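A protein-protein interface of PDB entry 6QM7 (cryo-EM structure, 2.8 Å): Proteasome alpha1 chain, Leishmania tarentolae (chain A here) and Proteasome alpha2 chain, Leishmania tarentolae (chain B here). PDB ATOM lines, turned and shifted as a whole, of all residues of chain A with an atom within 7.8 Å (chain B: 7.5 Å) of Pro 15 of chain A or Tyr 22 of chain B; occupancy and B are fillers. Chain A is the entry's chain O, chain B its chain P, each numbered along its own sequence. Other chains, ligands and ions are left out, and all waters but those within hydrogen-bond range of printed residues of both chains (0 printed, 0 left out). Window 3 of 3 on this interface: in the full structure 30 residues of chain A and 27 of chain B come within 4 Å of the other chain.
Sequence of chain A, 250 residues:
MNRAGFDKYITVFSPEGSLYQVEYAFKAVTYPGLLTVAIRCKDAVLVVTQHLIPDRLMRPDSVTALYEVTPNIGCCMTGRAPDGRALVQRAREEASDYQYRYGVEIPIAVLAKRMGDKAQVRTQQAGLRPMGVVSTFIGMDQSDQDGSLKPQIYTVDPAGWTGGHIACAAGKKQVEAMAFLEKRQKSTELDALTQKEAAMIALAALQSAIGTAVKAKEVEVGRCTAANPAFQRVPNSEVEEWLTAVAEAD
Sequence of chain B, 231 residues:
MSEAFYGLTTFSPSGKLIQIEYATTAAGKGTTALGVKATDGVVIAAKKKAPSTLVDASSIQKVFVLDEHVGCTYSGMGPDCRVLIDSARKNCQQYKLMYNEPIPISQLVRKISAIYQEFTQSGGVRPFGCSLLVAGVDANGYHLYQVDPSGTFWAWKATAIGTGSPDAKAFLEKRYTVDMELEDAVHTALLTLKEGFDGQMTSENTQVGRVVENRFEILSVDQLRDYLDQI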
ATOM      1  N   ASP A   7      20.612  18.169  15.842  1.00  0.00           N
ATOM      2  CA  ASP A   7      20.948  17.762  14.449  1.00  0.00           C
ATOM      3  C   ASP A   7      20.661  16.269  14.249  1.00  0.00           C
ATOM      4  O   ASP A   7      20.369  15.874  13.100  1.00  0.00           O
ATOM      5  CB  ASP A   7      22.431  18.001  14.126  1.00  0.00           C
ATOM      6  CG  ASP A   7      22.917  19.438  14.261  1.00  0.00           C
ATOM      7  OD1 ASP A   7      22.270  20.339  13.690  1.00  0.00           O
ATOM      8  OD2 ASP A   7      23.953  19.639  14.926  1.00  0.00           O
ATOM      9  N   VAL A  12      17.662  17.187   9.721  1.00  0.00           N
ATOM     10  CA  VAL A  12      18.259  18.509   9.396  1.00  0.00           C
ATOM     11  C   VAL A  12      19.759  18.313   9.206  1.00  0.00           C
ATOM     12  O   VAL A  12      20.335  17.369   9.798  1.00  0.00           O
ATOM     13  CB  VAL A  12      17.978  19.556  10.487  1.00  0.00           C
ATOM     14  CG1 VAL A  12      16.499  19.862  10.596  1.00  0.00           C
ATOM     15  CG2 VAL A  12      18.542  19.152  11.833  1.00  0.00           C
ATOM     16  N   PHE A  13      20.362  19.188   8.417  1.00  0.00           N
ATOM     17  CA  PHE A  13      21.815  19.196   8.178  1.00  0.00           C
ATOM     18  C   PHE A  13      22.527  19.474   9.489  1.00  0.00           C
ATOM     19  O   PHE A  13      22.036  20.276  10.298  1.00  0.00           O
ATOM     20  CB  PHE A  13      22.181  20.221   7.116  1.00  0.00           C
ATOM     21  CG  PHE A  13      21.632  19.852   5.770  1.00  0.00           C
ATOM     22  CD1 PHE A  13      22.254  18.884   5.002  1.00  0.00           C
ATOM     23  CD2 PHE A  13      20.462  20.427   5.310  1.00  0.00           C
ATOM     24  CE1 PHE A  13      21.735  18.523   3.774  1.00  0.00           C
ATOM     25  CE2 PHE A  13      19.940  20.064   4.084  1.00  0.00           C
ATOM     26  CZ  PHE A  13      20.576  19.113   3.317  1.00  0.00           C
ATOM     27  N   SER A  14      23.627  18.756   9.696  1.00  0.00           N
ATOM     28  CA  SER A  14      24.671  19.049  10.699  1.00  0.00           C
ATOM     29  C   SER A  14      25.520  20.192  10.161  1.00  0.00           C
ATOM     30  O   SER A  14      25.427  20.508   8.983  1.00  0.00           O
ATOM     31  CB  SER A  14      25.487  17.817  10.958  1.00  0.00           C
ATOM     32  OG  SER A  14      26.270  17.468   9.823  1.00  0.00           O
ATOM     33  N   PRO A  15      26.378  20.836  10.981  1.00  0.00           N
ATOM     34  CA  PRO A  15      27.295  21.853  10.462  1.00  0.00           C
ATOM     35  C   PRO A  15      28.205  21.387   9.315  1.00  0.00           C
ATOM     36  O   PRO A  15      28.566  22.219   8.504  1.00  0.00           O
ATOM     37  CB  PRO A  15      28.111  22.241  11.704  1.00  0.00           C
ATOM     38  CG  PRO A  15      27.162  21.961  12.862  1.00  0.00           C
ATOM     39  CD  PRO A  15      26.456  20.688  12.446  1.00  0.00           C
ATOM     40  N   GLU A  16      28.505  20.087   9.240  1.00  0.00           N
ATOM     41  CA  GLU A  16      29.379  19.483   8.192  1.00  0.00           C
ATOM     42  C   GLU A  16      28.500  18.892   7.077  1.00  0.00           C
ATOM     43  O   GLU A  16      28.971  17.998   6.361  1.00  0.00           O
ATOM     44  CB  GLU A  16      30.375  18.481   8.803  1.00  0.00           C
ATOM     45  CG  GLU A  16      29.824  17.595   9.920  1.00  0.00           C
ATOM     46  CD  GLU A  16      29.768  18.208  11.317  1.00  0.00           C
ATOM     47  OE1 GLU A  16      30.291  19.332  11.512  1.00  0.00           O
ATOM     48  OE2 GLU A  16      29.181  17.563  12.214  1.00  0.00           O
ATOM     49  N   GLY A  17      27.265  19.388   6.933  1.00  0.00           N
ATOM     50  CA  GLY A  17      26.396  19.191   5.756  1.00  0.00           C
ATOM     51  C   GLY A  17      25.870  17.776   5.621  1.00  0.00           C
ATOM     52  O   GLY A  17      25.493  17.406   4.496  1.00  0.00           O
ATOM     53  N   SER A  18      25.811  17.020   6.717  1.00  0.00           N
ATOM     54  CA  SER A  18      25.415  15.587   6.736  1.00  0.00           C
ATOM     55  C   SER A  18      24.078  15.430   7.460  1.00  0.00           C
ATOM     56  O   SER A  18      23.780  16.259   8.332  1.00  0.00           O
ATOM     57  CB  SER A  18      26.499  14.731   7.361  1.00  0.00           C
ATOM     58  OG  SER A  18      26.622  14.964   8.763  1.00  0.00           O
ATOM     59  N   TYR A  20      22.408  13.085   9.963  1.00  0.00           N
ATOM     60  CA  TYR A  20      22.846  12.031  10.912  1.00  0.00           C
ATOM     61  C   TYR A  20      21.839  10.877  10.892  1.00  0.00           C
ATOM     62  O   TYR A  20      22.280   9.727  10.923  1.00  0.00           O
ATOM     63  CB  TYR A  20      23.076  12.600  12.315  1.00  0.00           C
ATOM     64  CG  TYR A  20      24.424  13.248  12.511  1.00  0.00           C
ATOM     65  CD1 TYR A  20      25.597  12.537  12.302  1.00  0.00           C
ATOM     66  CD2 TYR A  20      24.534  14.571  12.911  1.00  0.00           C
ATOM     67  CE1 TYR A  20      26.843  13.123  12.474  1.00  0.00           C
ATOM     68  CE2 TYR A  20      25.770  15.169  13.103  1.00  0.00           C
ATOM     69  CZ  TYR A  20      26.931  14.446  12.875  1.00  0.00           C
ATOM     70  OH  TYR A  20      28.150  15.036  13.051  1.00  0.00           O
ATOM     71  N   SER B  12      19.149  32.831  12.910  1.00  0.00           N
ATOM     72  CA  SER B  12      20.072  32.981  14.064  1.00  0.00           C
ATOM     73  C   SER B  12      20.046  34.431  14.519  1.00  0.00           C
ATOM     74  O   SER B  12      19.698  35.307  13.739  1.00  0.00           O
ATOM     75  CB  SER B  12      21.481  32.593  13.695  1.00  0.00           C
ATOM     76  OG  SER B  12      21.526  31.259  13.217  1.00  0.00           O
ATOM     77  N   LEU B  17      20.513  32.270   8.065  1.00  0.00           N
ATOM     78  CA  LEU B  17      19.682  31.043   8.067  1.00  0.00           C
ATOM     79  C   LEU B  17      20.636  29.850   8.093  1.00  0.00           C
ATOM     80  O   LEU B  17      21.106  29.431   7.037  1.00  0.00           O
ATOM     81  CB  LEU B  17      18.776  31.027   6.836  1.00  0.00           C
ATOM     82  CG  LEU B  17      17.706  32.113   6.806  1.00  0.00           C
ATOM     83  CD1 LEU B  17      17.113  32.271   5.415  1.00  0.00           C
ATOM     84  CD2 LEU B  17      16.609  31.806   7.815  1.00  0.00           C
ATOM     85  N   ILE B  18      20.918  29.365   9.293  1.00  0.00           N
ATOM     86  CA  ILE B  18      21.985  28.371   9.589  1.00  0.00           C
ATOM     87  C   ILE B  18      21.736  27.098   8.775  1.00  0.00           C
ATOM     88  O   ILE B  18      22.715  26.535   8.279  1.00  0.00           O
ATOM     89  CB  ILE B  18      22.073  28.143  11.119  1.00  0.00           C
ATOM     90  CG1 ILE B  18      23.170  29.011  11.742  1.00  0.00           C
ATOM     91  CG2 ILE B  18      22.249  26.681  11.487  1.00  0.00           C
ATOM     92  CD1 ILE B  18      24.568  28.764  11.176  1.00  0.00           C
ATOM     93  N   GLN B  19      20.489  26.670   8.620  1.00  0.00           N
ATOM     94  CA  GLN B  19      20.175  25.376   7.961  1.00  0.00           C
ATOM     95  C   GLN B  19      20.421  25.494   6.456  1.00  0.00           C
ATOM     96  O   GLN B  19      20.691  24.456   5.852  1.00  0.00           O
ATOM     97  CB  GLN B  19      18.744  24.930   8.282  1.00  0.00           C
ATOM     98  CG  GLN B  19      18.594  23.433   8.543  1.00  0.00           C
ATOM     99  CD  GLN B  19      19.520  22.950   9.630  1.00  0.00           C
ATOM    100  OE1 GLN B  19      19.694  23.590  10.668  1.00  0.00           O
ATOM    101  NE2 GLN B  19      20.151  21.822   9.377  1.00  0.00           N
ATOM    102  N   ILE B  20      20.353  26.699   5.879  1.00  0.00           N
ATOM    103  CA  ILE B  20      20.691  26.974   4.446  1.00  0.00           C
ATOM    104  C   ILE B  20      22.212  27.056   4.269  1.00  0.00           C
ATOM    105  O   ILE B  20      22.689  26.708   3.181  1.00  0.00           O
ATOM    106  CB  ILE B  20      20.008  28.258   3.946  1.00  0.00           C
ATOM    107  CG1 ILE B  20      18.486  28.133   3.982  1.00  0.00           C
ATOM    108  CG2 ILE B  20      20.485  28.627   2.554  1.00  0.00           C
ATOM    109  CD1 ILE B  20      17.766  29.445   3.748  1.00  0.00           C
ATOM    110  N   GLU B  21      22.941  27.539   5.272  1.00  0.00           N
ATOM    111  CA  GLU B  21      24.425  27.550   5.253  1.00  0.00           C
ATOM    112  C   GLU B  21      24.926  26.111   5.265  1.00  0.00           C
ATOM    113  O   GLU B  21      25.899  25.819   4.552  1.00  0.00           O
ATOM    114  CB  GLU B  21      25.002  28.317   6.442  1.00  0.00           C
ATOM    115  CG  GLU B  21      24.838  29.823   6.326  1.00  0.00           C
ATOM    116  CD  GLU B  21      25.816  30.620   7.182  1.00  0.00           C
ATOM    117  OE1 GLU B  21      26.196  31.742   6.765  1.00  0.00           O
ATOM    118  OE2 GLU B  21      26.208  30.108   8.262  1.00  0.00           O
ATOM    119  N   TYR B  22      24.282  25.263   6.061  1.00  0.00           N
ATOM    120  CA  TYR B  22      24.663  23.843   6.252  1.00  0.00           C
ATOM    121  C   TYR B  22      24.293  23.045   5.002  1.00  0.00           C
ATOM    122  O   TYR B  22      25.061  22.162   4.611  1.00  0.00           O
ATOM    123  CB  TYR B  22      24.023  23.278   7.520  1.00  0.00           C
ATOM    124  CG  TYR B  22      24.511  23.852   8.835  1.00  0.00           C
ATOM    125  CD1 TYR B  22      25.631  24.675   8.924  1.00  0.00           C
ATOM    126  CD2 TYR B  22      23.865  23.518  10.017  1.00  0.00           C
ATOM    127  CE1 TYR B  22      26.064  25.175  10.142  1.00  0.00           C
ATOM    128  CE2 TYR B  22      24.287  24.005  11.241  1.00  0.00           C
ATOM    129  CZ  TYR B  22      25.390  24.841  11.307  1.00  0.00           C
ATOM    130  OH  TYR B  22      25.807  25.322  12.518  1.00  0.00           O
ATOM    131  N   ALA B  23      23.163  23.349   4.377  1.00  0.00           N
ATOM    132  CA  ALA B  23      22.760  22.698   3.117  1.00  0.00           C
ATOM    133  C   ALA B  23      23.741  23.100   2.011  1.00  0.00           C
ATOM    134  O   ALA B  23      24.026  22.270   1.142  1.00  0.00           O
ATOM    135  CB  ALA B  23      21.338  23.059   2.769  1.00  0.00           C
ATOM    136  N   THR B  24      24.227  24.339   2.027  1.00  0.00           N
ATOM    137  CA  THR B  24      25.204  24.847   1.030  1.00  0.00           C
ATOM    138  C   THR B  24      26.540  24.131   1.251  1.00  0.00           C
ATOM    139  O   THR B  24      27.260  23.927   0.260  1.00  0.00           O
ATOM    140  CB  THR B  24      25.253  26.380   1.042  1.00  0.00           C
ATOM    141  OG1 THR B  24      24.044  26.828   0.423  1.00  0.00           O
ATOM    142  CG2 THR B  24      26.443  26.950   0.300  1.00  0.00           C
ATOM    143  N   THR B  25      26.840  23.729   2.485  1.00  0.00           N
ATOM    144  CA  THR B  25      28.005  22.873   2.806  1.00  0.00           C
ATOM    145  C   THR B  25      27.802  21.494   2.176  1.00  0.00           C
ATOM    146  O   THR B  25      28.752  20.985   1.565  1.00  0.00           O
ATOM    147  CB  THR B  25      28.240  22.802   4.314  1.00  0.00           C
ATOM    148  OG1 THR B  25      28.443  24.145   4.763  1.00  0.00           O
ATOM    149  CG2 THR B  25      29.428  21.932   4.663  1.00  0.00           C
ATOM    150  N   ALA B  26      26.600  20.935   2.305  1.00  0.00           N
ATOM    151  CA  ALA B  26      26.196  19.637   1.712  1.00  0.00           C
ATOM    152  C   ALA B  26      26.390  19.665   0.201  1.00  0.00           C
ATOM    153  O   ALA B  26      26.762  18.606  -0.349  1.00  0.00           O
ATOM    154  CB  ALA B  26      24.759  19.304   2.033  1.00  0.00           C
ATOM    155  N   ALA B  27      26.102  20.804  -0.432  1.00  0.00           N
ATOM    156  CA  ALA B  27      26.152  20.990  -1.901  1.00  0.00           C
ATOM    157  C   ALA B  27      27.608  21.126  -2.352  1.00  0.00           C
ATOM    158  O   ALA B  27      27.917  20.687  -3.464  1.00  0.00           O
ATOM    159  CB  ALA B  27      25.315  22.174  -2.317  1.00  0.00           C
ATOM    160  N   GLY B  28      28.474  21.688  -1.516  1.00  0.00           N
ATOM    161  CA  GLY B  28      29.911  21.810  -1.827  1.00  0.00           C
ATOM    162  C   GLY B  28      30.638  20.474  -1.764  1.00  0.00           C
ATOM    163  O   GLY B  28      31.768  20.407  -2.279  1.00  0.00           O
ATOM    164  N   LYS B  29      30.035  19.458  -1.135  1.00  0.00           N
ATOM    165  CA  LYS B  29      30.709  18.194  -0.730  1.00  0.00           C
ATOM    166  C   LYS B  29      30.609  17.154  -1.850  1.00  0.00           C
ATOM    167  O   LYS B  29      31.406  16.191  -1.821  1.00  0.00           O
ATOM    168  CB  LYS B  29      30.121  17.661   0.582  1.00  0.00           C
ATOM    169  CG  LYS B  29      31.012  17.812   1.813  1.00  0.00           C
ATOM    170  CD  LYS B  29      30.259  17.954   3.137  1.00  0.00           C
ATOM    171  CE  LYS B  29      29.092  16.995   3.336  1.00  0.00           C
ATOM    172  NZ  LYS B  29      29.418  15.874   4.250  1.00  0.00           N
ATOM    173  N   PRO B 127      16.116  22.219   3.845  1.00  0.00           N
ATOM    174  CA  PRO B 127      16.477  22.615   2.492  1.00  0.00           C
ATOM    175  C   PRO B 127      17.096  21.478   1.666  1.00  0.00           C
ATOM    176  O   PRO B 127      17.482  20.463   2.223  1.00  0.00           O
ATOM    177  CB  PRO B 127      17.564  23.679   2.696  1.00  0.00           C
ATOM    178  CG  PRO B 127      17.334  24.160   4.086  1.00  0.00           C
ATOM    179  CD  PRO B 127      16.941  22.913   4.842  1.00  0.00           C
ATOM    180  N   PHE B 128      17.177  21.676   0.351  1.00  0.00           N
ATOM    181  CA  PHE B 128      17.884  20.750  -0.553  1.00  0.00           C
ATOM    182  C   PHE B 128      19.380  20.938  -0.346  1.00  0.00           C
ATOM    183  O   PHE B 128      19.812  22.094  -0.249  1.00  0.00           O
ATOM    184  CB  PHE B 128      17.507  21.006  -2.002  1.00  0.00           C
ATOM    185  CG  PHE B 128      16.075  20.671  -2.293  1.00  0.00           C
ATOM    186  CD1 PHE B 128      15.698  19.384  -2.620  1.00  0.00           C
ATOM    187  CD2 PHE B 128      15.103  21.651  -2.224  1.00  0.00           C
ATOM    188  CE1 PHE B 128      14.373  19.087  -2.896  1.00  0.00           C
ATOM    189  CE2 PHE B 128      13.779  21.347  -2.490  1.00  0.00           C
ATOM    190  CZ  PHE B 128      13.414  20.066  -2.827  1.00  0.00           C
ATOM    191  N   GLY B 129      20.117  19.833  -0.263  1.00  0.00           N
ATOM    192  CA  GLY B 129      21.576  19.845  -0.115  1.00  0.00           C
ATOM    193  C   GLY B 129      22.247  19.642  -1.450  1.00  0.00           C
ATOM    194  O   GLY B 129      23.125  18.775  -1.546  1.00  0.00           O
ATOM    195  N   PRO B 149      21.152  25.838  -2.732  1.00  0.00           N
ATOM    196  CA  PRO B 149      20.186  25.497  -1.690  1.00  0.00           C
ATOM    197  C   PRO B 149      19.327  26.646  -1.151  1.00  0.00           C
ATOM    198  O   PRO B 149      18.206  26.367  -0.752  1.00  0.00           O
ATOM    199  CB  PRO B 149      21.114  24.988  -0.585  1.00  0.00           C
ATOM    200  CG  PRO B 149      22.163  24.260  -1.369  1.00  0.00           C
ATOM    201  CD  PRO B 149      22.471  25.231  -2.484  1.00  0.00           C
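NE2 of Gln 19 of chain B sits at hydrogen-bond distance from O of Phe 13 of chain A (2.6 Å). NZ of Lys 29 of chain B is in hydrogen-bond range of O of Glu 16 of chain A (3.0 Å).
The side-chain hydroxyl of Ser 14 of chain A lies close to the backbone NH of Glu 16 of chain A (3.5 Å). OG of Ser 14 of chain A lies within hydrogen-bond range of OG of Ser 18 of chain A, at 2.7 Å. The side-chain carboxylate of Glu 16 of chain A sits at hydrogen-bond distance from the side-chain hydroxyl of Tyr 20 of chain A (2.9 Å). The side-chain hydroxyl (OG1) of Thr 25 of chain B lies within hydrogen-bond range of the backbone carbonyl oxygen (O) of Glu 21 of chain B, at 3.1 Å.
Among the printed residues, merely in contact across the chains: Phe 13 of chain A with Pro 127 of chain B (3.1 Å), Gly 17 of chain A with Ala 26 of chain B (3.2 Å), Val 12 of chain A with Gln 19 of chain B (3.3 Å), Ser 14 of chain A with Tyr 22 of chain B (3.4 Å), Gly 17 of chain A with Tyr 22 of chain B (3.5 Å), Pro 15 of chain A with Tyr 22 of chain B (3.6 Å), Phe 13 of chain A with Ala 23 of chain B (3.6 Å), Phe 13 of chain A with Ala 26 of chain B (3.6 Å), Phe 13 of chain A with Tyr 22 of chain B (3.6 Å), Phe 13 of chain A with Gly 129 of chain B (3.6 Å), Gly 17 of chain A with Lys 29 of chain B (3.8 Å), Pro 15 of chain A with Thr 25 of chain B (3.9 Å) and Glu 16 of chain A with Thr 25 of chain B (3.99 Å).
Of the printed residues of chain B, Phe 13 of chain A touches Gln 19 (2.6 Å), Tyr 22 (3.6 Å), Ala 23 (3.6 Å), Ala 26 (3.6 Å), Pro 127 (3.1 Å) and Gly 129 (3.6 Å). Printed residues of chain B within 4 Å of Ser 14 of chain A: Tyr 22 (3.4 Å). Tyr 22 of chain B touches just these residues of chain A: Phe 13, Ser 14, Pro 15 and Gly 17. Of chain A, only Phe 13 comes within 4 Å of Ala 23 of chain B. Of the printed residues of chain A, Ala 26 of chain B touches Phe 13 and Gly 17.
Of the 9 printed residues of chain A, 6 touch a printed residue of chain B. Hydrophobic or aromatic side chains of chain A that line the printed part of chain B: Val 12, Phe 13 and Pro 15. Of the 18 printed residues of chain B, 8 touch a printed residue of chain A. Hydrophobic or aromatic side chains of chain B that line the printed part of chain A: Tyr 22, Ala 23 and Ala 26. Among the printed residues, 15 pairs touch across the chains.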
